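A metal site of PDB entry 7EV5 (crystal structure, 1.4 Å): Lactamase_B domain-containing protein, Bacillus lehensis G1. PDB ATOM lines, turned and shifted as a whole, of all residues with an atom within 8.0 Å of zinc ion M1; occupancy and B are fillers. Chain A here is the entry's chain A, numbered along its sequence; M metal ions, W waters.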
ATOM      1  N   THR A  12      -3.590  17.616  -5.425  1.00  0.00           N
ATOM      2  CA  THR A  12      -2.383  18.363  -5.100  1.00  0.00           C
ATOM      3  C   THR A  12      -2.495  19.791  -5.596  1.00  0.00           C
ATOM      4  O   THR A  12      -2.971  20.048  -6.713  1.00  0.00           O
ATOM      5  CB  THR A  12      -1.206  17.683  -5.785  1.00  0.00           C
ATOM      6  OG1 THR A  12      -1.128  16.322  -5.319  1.00  0.00           O
ATOM      7  CG2 THR A  12       0.125  18.380  -5.461  1.00  0.00           C
ATOM      8  N   ASP A  28       4.394  23.113  -9.430  1.00  0.00           N
ATOM      9  CA  ASP A  28       3.825  21.794  -9.202  1.00  0.00           C
ATOM     10  C   ASP A  28       2.541  21.497  -9.985  1.00  0.00           C
ATOM     11  O   ASP A  28       1.493  21.232  -9.383  1.00  0.00           O
ATOM     12  CB  ASP A  28       3.585  21.558  -7.709  1.00  0.00           C
ATOM     13  CG  ASP A  28       4.873  21.510  -6.906  1.00  0.00           C
ATOM     14  OD1 ASP A  28       5.965  21.722  -7.461  1.00  0.00           O
ATOM     15  OD2 ASP A  28       4.782  21.271  -5.681  1.00  0.00           O
ATOM     16  N   THR A  53       8.599  21.895  -6.508  1.00  0.00           N
ATOM     17  CA  THR A  53       9.075  21.710  -5.149  1.00  0.00           C
ATOM     18  C   THR A  53       9.742  20.358  -4.991  1.00  0.00           C
ATOM     19  O   THR A  53      10.720  20.221  -4.230  1.00  0.00           O
ATOM     20  CB  THR A  53       7.938  21.869  -4.128  1.00  0.00           C
ATOM     21  OG1 THR A  53       6.979  20.813  -4.291  1.00  0.00           O
ATOM     22  CG2 THR A  53       7.266  23.213  -4.258  1.00  0.00           C
ATOM     23  N   HIS A  54       9.223  19.348  -5.680  1.00  0.00           N
ATOM     24  CA  HIS A  54       9.757  17.991  -5.686  1.00  0.00           C
ATOM     25  C   HIS A  54       9.078  17.225  -6.813  1.00  0.00           C
ATOM     26  O   HIS A  54       8.154  17.730  -7.459  1.00  0.00           O
ATOM     27  CB  HIS A  54       9.663  17.295  -4.315  1.00  0.00           C
ATOM     28  CG  HIS A  54       8.263  16.990  -3.823  1.00  0.00           C
ATOM     29  ND1 HIS A  54       7.292  17.948  -3.655  1.00  0.00           N
ATOM     30  CD2 HIS A  54       7.735  15.829  -3.374  1.00  0.00           C
ATOM     31  CE1 HIS A  54       6.201  17.380  -3.146  1.00  0.00           C
ATOM     32  NE2 HIS A  54       6.437  16.098  -2.976  1.00  0.00           N
ATOM     33  N   ALA A  55       9.542  15.997  -7.028  1.00  0.00           N
ATOM     34  CA  ALA A  55       9.154  15.250  -8.220  1.00  0.00           C
ATOM     35  C   ALA A  55       8.287  14.038  -7.924  1.00  0.00           C
ATOM     36  O   ALA A  55       8.222  13.105  -8.738  1.00  0.00           O
ATOM     37  CB  ALA A  55      10.376  14.863  -9.057  1.00  0.00           C
ATOM     38  N   HIS A  56       7.612  14.016  -6.781  1.00  0.00           N
ATOM     39  CA  HIS A  56       6.583  13.001  -6.598  1.00  0.00           C
ATOM     40  C   HIS A  56       5.543  13.107  -7.707  1.00  0.00           C
ATOM     41  O   HIS A  56       5.233  14.203  -8.197  1.00  0.00           O
ATOM     42  CB  HIS A  56       5.901  13.156  -5.237  1.00  0.00           C
ATOM     43  CG  HIS A  56       6.667  12.537  -4.114  1.00  0.00           C
ATOM     44  ND1 HIS A  56       6.553  12.987  -2.816  1.00  0.00           N
ATOM     45  CD2 HIS A  56       7.535  11.510  -4.079  1.00  0.00           C
ATOM     46  CE1 HIS A  56       7.323  12.259  -2.028  1.00  0.00           C
ATOM     47  NE2 HIS A  56       7.933  11.356  -2.779  1.00  0.00           N
ATOM     48  N   PHE A  57       4.972  11.950  -8.068  1.00  0.00           N
ATOM     49  CA  PHE A  57       4.080  11.878  -9.220  1.00  0.00           C
ATOM     50  C   PHE A  57       2.923  12.879  -9.137  1.00  0.00           C
ATOM     51  O   PHE A  57       2.462  13.390 -10.159  1.00  0.00           O
ATOM     52  CB  PHE A  57       3.529  10.447  -9.358  1.00  0.00           C
ATOM     53  CG  PHE A  57       2.505  10.092  -8.301  1.00  0.00           C
ATOM     54  CD1 PHE A  57       1.136  10.215  -8.560  1.00  0.00           C
ATOM     55  CD2 PHE A  57       2.905   9.645  -7.051  1.00  0.00           C
ATOM     56  CE1 PHE A  57       0.202   9.901  -7.580  1.00  0.00           C
ATOM     57  CE2 PHE A  57       1.981   9.330  -6.070  1.00  0.00           C
ATOM     58  CZ  PHE A  57       0.626   9.463  -6.334  1.00  0.00           C
ATOM     59  N   ASP A  58       2.406  13.141  -7.927  1.00  0.00           N
ATOM     60  CA  ASP A  58       1.244  13.996  -7.781  1.00  0.00           C
ATOM     61  C   ASP A  58       1.562  15.463  -7.994  1.00  0.00           C
ATOM     62  O   ASP A  58       0.644  16.284  -8.023  1.00  0.00           O
ATOM     63  CB  ASP A  58       0.569  13.750  -6.426  1.00  0.00           C
ATOM     64  CG  ASP A  58       1.484  14.019  -5.236  1.00  0.00           C
ATOM     65  OD1 ASP A  58       2.566  13.383  -5.166  1.00  0.00           O
ATOM     66  OD2 ASP A  58       1.103  14.855  -4.376  1.00  0.00           O
ATOM     67  N   HIS A  59       2.842  15.796  -8.174  1.00  0.00           N
ATOM     68  CA  HIS A  59       3.264  17.164  -8.458  1.00  0.00           C
ATOM     69  C   HIS A  59       3.725  17.369  -9.886  1.00  0.00           C
ATOM     70  O   HIS A  59       4.043  18.504 -10.255  1.00  0.00           O
ATOM     71  CB  HIS A  59       4.361  17.596  -7.472  1.00  0.00           C
ATOM     72  CG  HIS A  59       3.904  17.580  -6.042  1.00  0.00           C
ATOM     73  ND1 HIS A  59       3.710  18.719  -5.294  1.00  0.00           N
ATOM     74  CD2 HIS A  59       3.528  16.545  -5.254  1.00  0.00           C
ATOM     75  CE1 HIS A  59       3.247  18.387  -4.103  1.00  0.00           C
ATOM     76  NE2 HIS A  59       3.113  17.070  -4.055  1.00  0.00           N
ATOM     77  N   GLU A  80      16.614  14.765  -7.270  1.00  0.00           N
ATOM     78  CA  GLU A  80      15.464  14.047  -7.819  1.00  0.00           C
ATOM     79  C   GLU A  80      15.431  14.062  -9.352  1.00  0.00           C
ATOM     80  O   GLU A  80      14.391  13.776  -9.948  1.00  0.00           O
ATOM     81  CB  GLU A  80      14.159  14.576  -7.232  1.00  0.00           C
ATOM     82  CG  GLU A  80      14.020  14.213  -5.756  1.00  0.00           C
ATOM     83  CD  GLU A  80      12.818  14.859  -5.085  1.00  0.00           C
ATOM     84  OE1 GLU A  80      11.887  15.288  -5.786  1.00  0.00           O
ATOM     85  OE2 GLU A  80      12.816  14.938  -3.838  1.00  0.00           O
ATOM     86  N   TRP A  83      13.825  11.235 -11.067  1.00  0.00           N
ATOM     87  CA  TRP A  83      12.475  10.854 -10.662  1.00  0.00           C
ATOM     88  C   TRP A  83      11.420  11.203 -11.694  1.00  0.00           C
ATOM     89  O   TRP A  83      10.367  10.548 -11.742  1.00  0.00           O
ATOM     90  CB  TRP A  83      12.110  11.559  -9.350  1.00  0.00           C
ATOM     91  CG  TRP A  83      12.806  11.009  -8.146  1.00  0.00           C
ATOM     92  CD1 TRP A  83      14.001  10.348  -8.115  1.00  0.00           C
ATOM     93  CD2 TRP A  83      12.360  11.093  -6.803  1.00  0.00           C
ATOM     94  NE1 TRP A  83      14.324  10.014  -6.816  1.00  0.00           N
ATOM     95  CE2 TRP A  83      13.316  10.446  -5.989  1.00  0.00           C
ATOM     96  CE3 TRP A  83      11.223  11.647  -6.209  1.00  0.00           C
ATOM     97  CZ2 TRP A  83      13.179  10.352  -4.595  1.00  0.00           C
ATOM     98  CZ3 TRP A  83      11.085  11.546  -4.827  1.00  0.00           C
ATOM     99  CH2 TRP A  83      12.066  10.894  -4.042  1.00  0.00           C
ATOM    100  N   ASN A  90       9.341   7.851  -8.451  1.00  0.00           N
ATOM    101  CA  ASN A  90       8.541   9.018  -8.117  1.00  0.00           C
ATOM    102  C   ASN A  90       7.273   8.690  -7.342  1.00  0.00           C
ATOM    103  O   ASN A  90       6.485   9.601  -7.077  1.00  0.00           O
ATOM    104  CB  ASN A  90       8.251   9.897  -9.350  1.00  0.00           C
ATOM    105  CG  ASN A  90       7.371   9.210 -10.399  1.00  0.00           C
ATOM    106  OD1 ASN A  90       6.505   8.395 -10.086  1.00  0.00           O
ATOM    107  ND2 ASN A  90       7.602   9.566 -11.659  1.00  0.00           N
ATOM    108  N   LEU A  95       2.454   3.655  -5.243  1.00  0.00           N
ATOM    109  CA  LEU A  95       1.325   4.195  -4.504  1.00  0.00           C
ATOM    110  C   LEU A  95       0.019   4.118  -5.272  1.00  0.00           C
ATOM    111  O   LEU A  95      -1.044   4.166  -4.648  1.00  0.00           O
ATOM    112  CB  LEU A  95       1.592   5.641  -4.078  1.00  0.00           C
ATOM    113  CG  LEU A  95       2.696   5.831  -3.032  1.00  0.00           C
ATOM    114  CD1 LEU A  95       2.920   7.318  -2.750  1.00  0.00           C
ATOM    115  CD2 LEU A  95       2.386   5.075  -1.740  1.00  0.00           C
ATOM    116  N   HIS A 131      10.646  15.030   3.558  1.00  0.00           N
ATOM    117  CA  HIS A 131       9.593  14.350   2.807  1.00  0.00           C
ATOM    118  C   HIS A 131      10.157  13.736   1.516  1.00  0.00           C
ATOM    119  O   HIS A 131       9.747  12.640   1.119  1.00  0.00           O
ATOM    120  CB  HIS A 131       8.452  15.334   2.528  1.00  0.00           C
ATOM    121  CG  HIS A 131       7.437  14.848   1.542  1.00  0.00           C
ATOM    122  ND1 HIS A 131       6.416  13.986   1.876  1.00  0.00           N
ATOM    123  CD2 HIS A 131       7.264  15.152   0.232  1.00  0.00           C
ATOM    124  CE1 HIS A 131       5.657  13.761   0.812  1.00  0.00           C
ATOM    125  NE2 HIS A 131       6.165  14.456  -0.205  1.00  0.00           N
ATOM    126  N   SER A 132      11.120  14.403   0.884  1.00  0.00           N
ATOM    127  CA  SER A 132      11.819  13.850  -0.257  1.00  0.00           C
ATOM    128  C   SER A 132      13.180  14.520  -0.337  1.00  0.00           C
ATOM    129  O   SER A 132      13.342  15.637   0.177  1.00  0.00           O
ATOM    130  CB  SER A 132      11.032  14.047  -1.578  1.00  0.00           C
ATOM    131  OG  SER A 132      11.038  15.386  -2.013  1.00  0.00           O
ATOM    132  N   SER A 135      13.451  17.997  -2.137  1.00  0.00           N
ATOM    133  CA  SER A 135      12.422  18.986  -1.802  1.00  0.00           C
ATOM    134  C   SER A 135      13.074  20.350  -1.600  1.00  0.00           C
ATOM    135  O   SER A 135      14.012  20.505  -0.807  1.00  0.00           O
ATOM    136  CB  SER A 135      11.738  18.592  -0.512  1.00  0.00           C
ATOM    137  OG  SER A 135      10.661  17.694  -0.717  1.00  0.00           O
ATOM    138  N   GLY A 149       5.914  23.101  -0.999  1.00  0.00           N
ATOM    139  CA  GLY A 149       5.627  21.710  -1.287  1.00  0.00           C
ATOM    140  C   GLY A 149       5.046  20.979  -0.083  1.00  0.00           C
ATOM    141  O   GLY A 149       4.130  21.457   0.585  1.00  0.00           O
ATOM    142  N   ASP A 150       5.593  19.787   0.193  1.00  0.00           N
ATOM    143  CA  ASP A 150       4.989  18.871   1.151  1.00  0.00           C
ATOM    144  C   ASP A 150       5.724  18.829   2.473  1.00  0.00           C
ATOM    145  O   ASP A 150       5.682  17.815   3.173  1.00  0.00           O
ATOM    146  CB  ASP A 150       4.849  17.474   0.541  1.00  0.00           C
ATOM    147  CG  ASP A 150       3.829  17.401  -0.583  1.00  0.00           C
ATOM    148  OD1 ASP A 150       3.245  18.453  -0.937  1.00  0.00           O
ATOM    149  OD2 ASP A 150       3.631  16.297  -1.121  1.00  0.00           O
ATOM    150  N   VAL A 151       6.383  19.925   2.855  1.00  0.00           N
ATOM    151  CA  VAL A 151       7.087  19.955   4.128  1.00  0.00           C
ATOM    152  C   VAL A 151       6.130  20.246   5.284  1.00  0.00           C
ATOM    153  O   VAL A 151       6.114  19.543   6.298  1.00  0.00           O
ATOM    154  CB  VAL A 151       8.217  20.986   4.053  1.00  0.00           C
ATOM    155  CG1 VAL A 151       8.853  21.202   5.408  1.00  0.00           C
ATOM    156  CG2 VAL A 151       9.275  20.527   3.048  1.00  0.00           C
ATOM    157  N   PHE A 153       2.086  21.548   6.315  1.00  0.00           N
ATOM    158  CA  PHE A 153       0.708  21.783   5.907  1.00  0.00           C
ATOM    159  C   PHE A 153      -0.008  22.503   7.029  1.00  0.00           C
ATOM    160  O   PHE A 153       0.508  22.666   8.134  1.00  0.00           O
ATOM    161  CB  PHE A 153      -0.023  20.456   5.657  1.00  0.00           C
ATOM    162  CG  PHE A 153       0.678  19.545   4.679  1.00  0.00           C
ATOM    163  CD1 PHE A 153       0.871  19.927   3.355  1.00  0.00           C
ATOM    164  CD2 PHE A 153       1.103  18.283   5.071  1.00  0.00           C
ATOM    165  CE1 PHE A 153       1.489  19.069   2.451  1.00  0.00           C
ATOM    166  CE2 PHE A 153       1.732  17.424   4.167  1.00  0.00           C
ATOM    167  CZ  PHE A 153       1.937  17.822   2.850  1.00  0.00           C
ATOM    168  N   GLY A 158       4.664  16.948   6.389  1.00  0.00           N
ATOM    169  CA  GLY A 158       4.811  15.978   5.320  1.00  0.00           C
ATOM    170  C   GLY A 158       5.048  14.568   5.835  1.00  0.00           C
ATOM    171  O   GLY A 158       5.718  14.345   6.850  1.00  0.00           O
ATOM    172  N   ARG A 159       4.501  13.595   5.108  1.00  0.00           N
ATOM    173  CA  ARG A 159       4.800  12.207   5.418  1.00  0.00           C
ATOM    174  C   ARG A 159       6.266  11.931   5.135  1.00  0.00           C
ATOM    175  O   ARG A 159       6.870  12.497   4.215  1.00  0.00           O
ATOM    176  CB  ARG A 159       3.898  11.256   4.619  1.00  0.00           C
ATOM    177  CG  ARG A 159       4.083  11.303   3.115  1.00  0.00           C
ATOM    178  CD  ARG A 159       2.932  10.617   2.396  1.00  0.00           C
ATOM    179  NE  ARG A 159       2.924   9.181   2.634  1.00  0.00           N
ATOM    180  CZ  ARG A 159       2.090   8.321   2.053  1.00  0.00           C
ATOM    181  NH1 ARG A 159       1.160   8.746   1.192  1.00  0.00           N
ATOM    182  NH2 ARG A 159       2.186   7.033   2.343  1.00  0.00           N
ATOM    183  N   LEU A 162       8.079   7.745   2.528  1.00  0.00           N
ATOM    184  CA  LEU A 162       8.301   7.462   1.117  1.00  0.00           C
ATOM    185  C   LEU A 162       9.803   7.359   0.805  1.00  0.00           C
ATOM    186  O   LEU A 162      10.643   7.348   1.702  1.00  0.00           O
ATOM    187  CB  LEU A 162       7.533   8.468   0.250  1.00  0.00           C
ATOM    188  CG  LEU A 162       6.044   8.643   0.565  1.00  0.00           C
ATOM    189  CD1 LEU A 162       5.382   9.681  -0.357  1.00  0.00           C
ATOM    190  CD2 LEU A 162       5.318   7.312   0.495  1.00  0.00           C
ATOM    191  N   GLY A 190       1.606  21.729  -0.697  1.00  0.00           N
ATOM    192  CA  GLY A 190       1.148  20.831  -1.745  1.00  0.00           C
ATOM    193  C   GLY A 190      -0.213  20.226  -1.499  1.00  0.00           C
ATOM    194  O   GLY A 190      -0.808  19.708  -2.445  1.00  0.00           O
ATOM    195  N   HIS A 191      -0.716  20.257  -0.266  1.00  0.00           N
ATOM    196  CA  HIS A 191      -1.967  19.558   0.027  1.00  0.00           C
ATOM    197  C   HIS A 191      -2.744  20.340   1.081  1.00  0.00           C
ATOM    198  O   HIS A 191      -2.178  20.710   2.107  1.00  0.00           O
ATOM    199  CB  HIS A 191      -1.670  18.133   0.527  1.00  0.00           C
ATOM    200  CG  HIS A 191      -0.910  17.304  -0.469  1.00  0.00           C
ATOM    201  ND1 HIS A 191      -1.532  16.558  -1.453  1.00  0.00           N
ATOM    202  CD2 HIS A 191       0.417  17.124  -0.657  1.00  0.00           C
ATOM    203  CE1 HIS A 191      -0.618  15.966  -2.195  1.00  0.00           C
ATOM    204  NE2 HIS A 191       0.572  16.294  -1.738  1.00  0.00           N
HETATM  205 ZN    ZN M   1       5.360  14.579  -2.099  1.00  0.00          ZN
HETATM  206 ZN    ZN M   2       2.331  15.816  -2.635  1.00  0.00          ZN
HETATM  207  O   HOH W   1       3.550  14.232  -2.711  1.00  0.00           O
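ND1 of His 59 sits at hydrogen-bond distance from OD2 of Asp 28. The backbone carbonyl oxygen (O) of Asp 150 sits close to the backbone NH (N) of Gly 158, 3.5 Å away. A ring nitrogen (ND1) of His 54 sits at hydrogen-bond distance from the side-chain hydroxyl of Thr 53. A ring nitrogen (ND1) of His 131 lies within hydrogen-bond range of the backbone carbonyl oxygen of Arg 159.
His 59 touches zinc ion M1 (NE2 to ZN, 3.9 Å). Of the 25 residues printed, 5 come within 4 Å of zinc ion M1.
Water W1 binds zinc ion M1. A ring nitrogen (NE2) of His 54 is bound to zinc ion M1. Zinc ion M1 is bound by NE2 of His 131. A ring nitrogen (ND1) of His 56 binds zinc ion M1 (2.1 Å). Slightly farther from zinc ion M1 lies OD2 of Asp 150 (2.6 Å).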
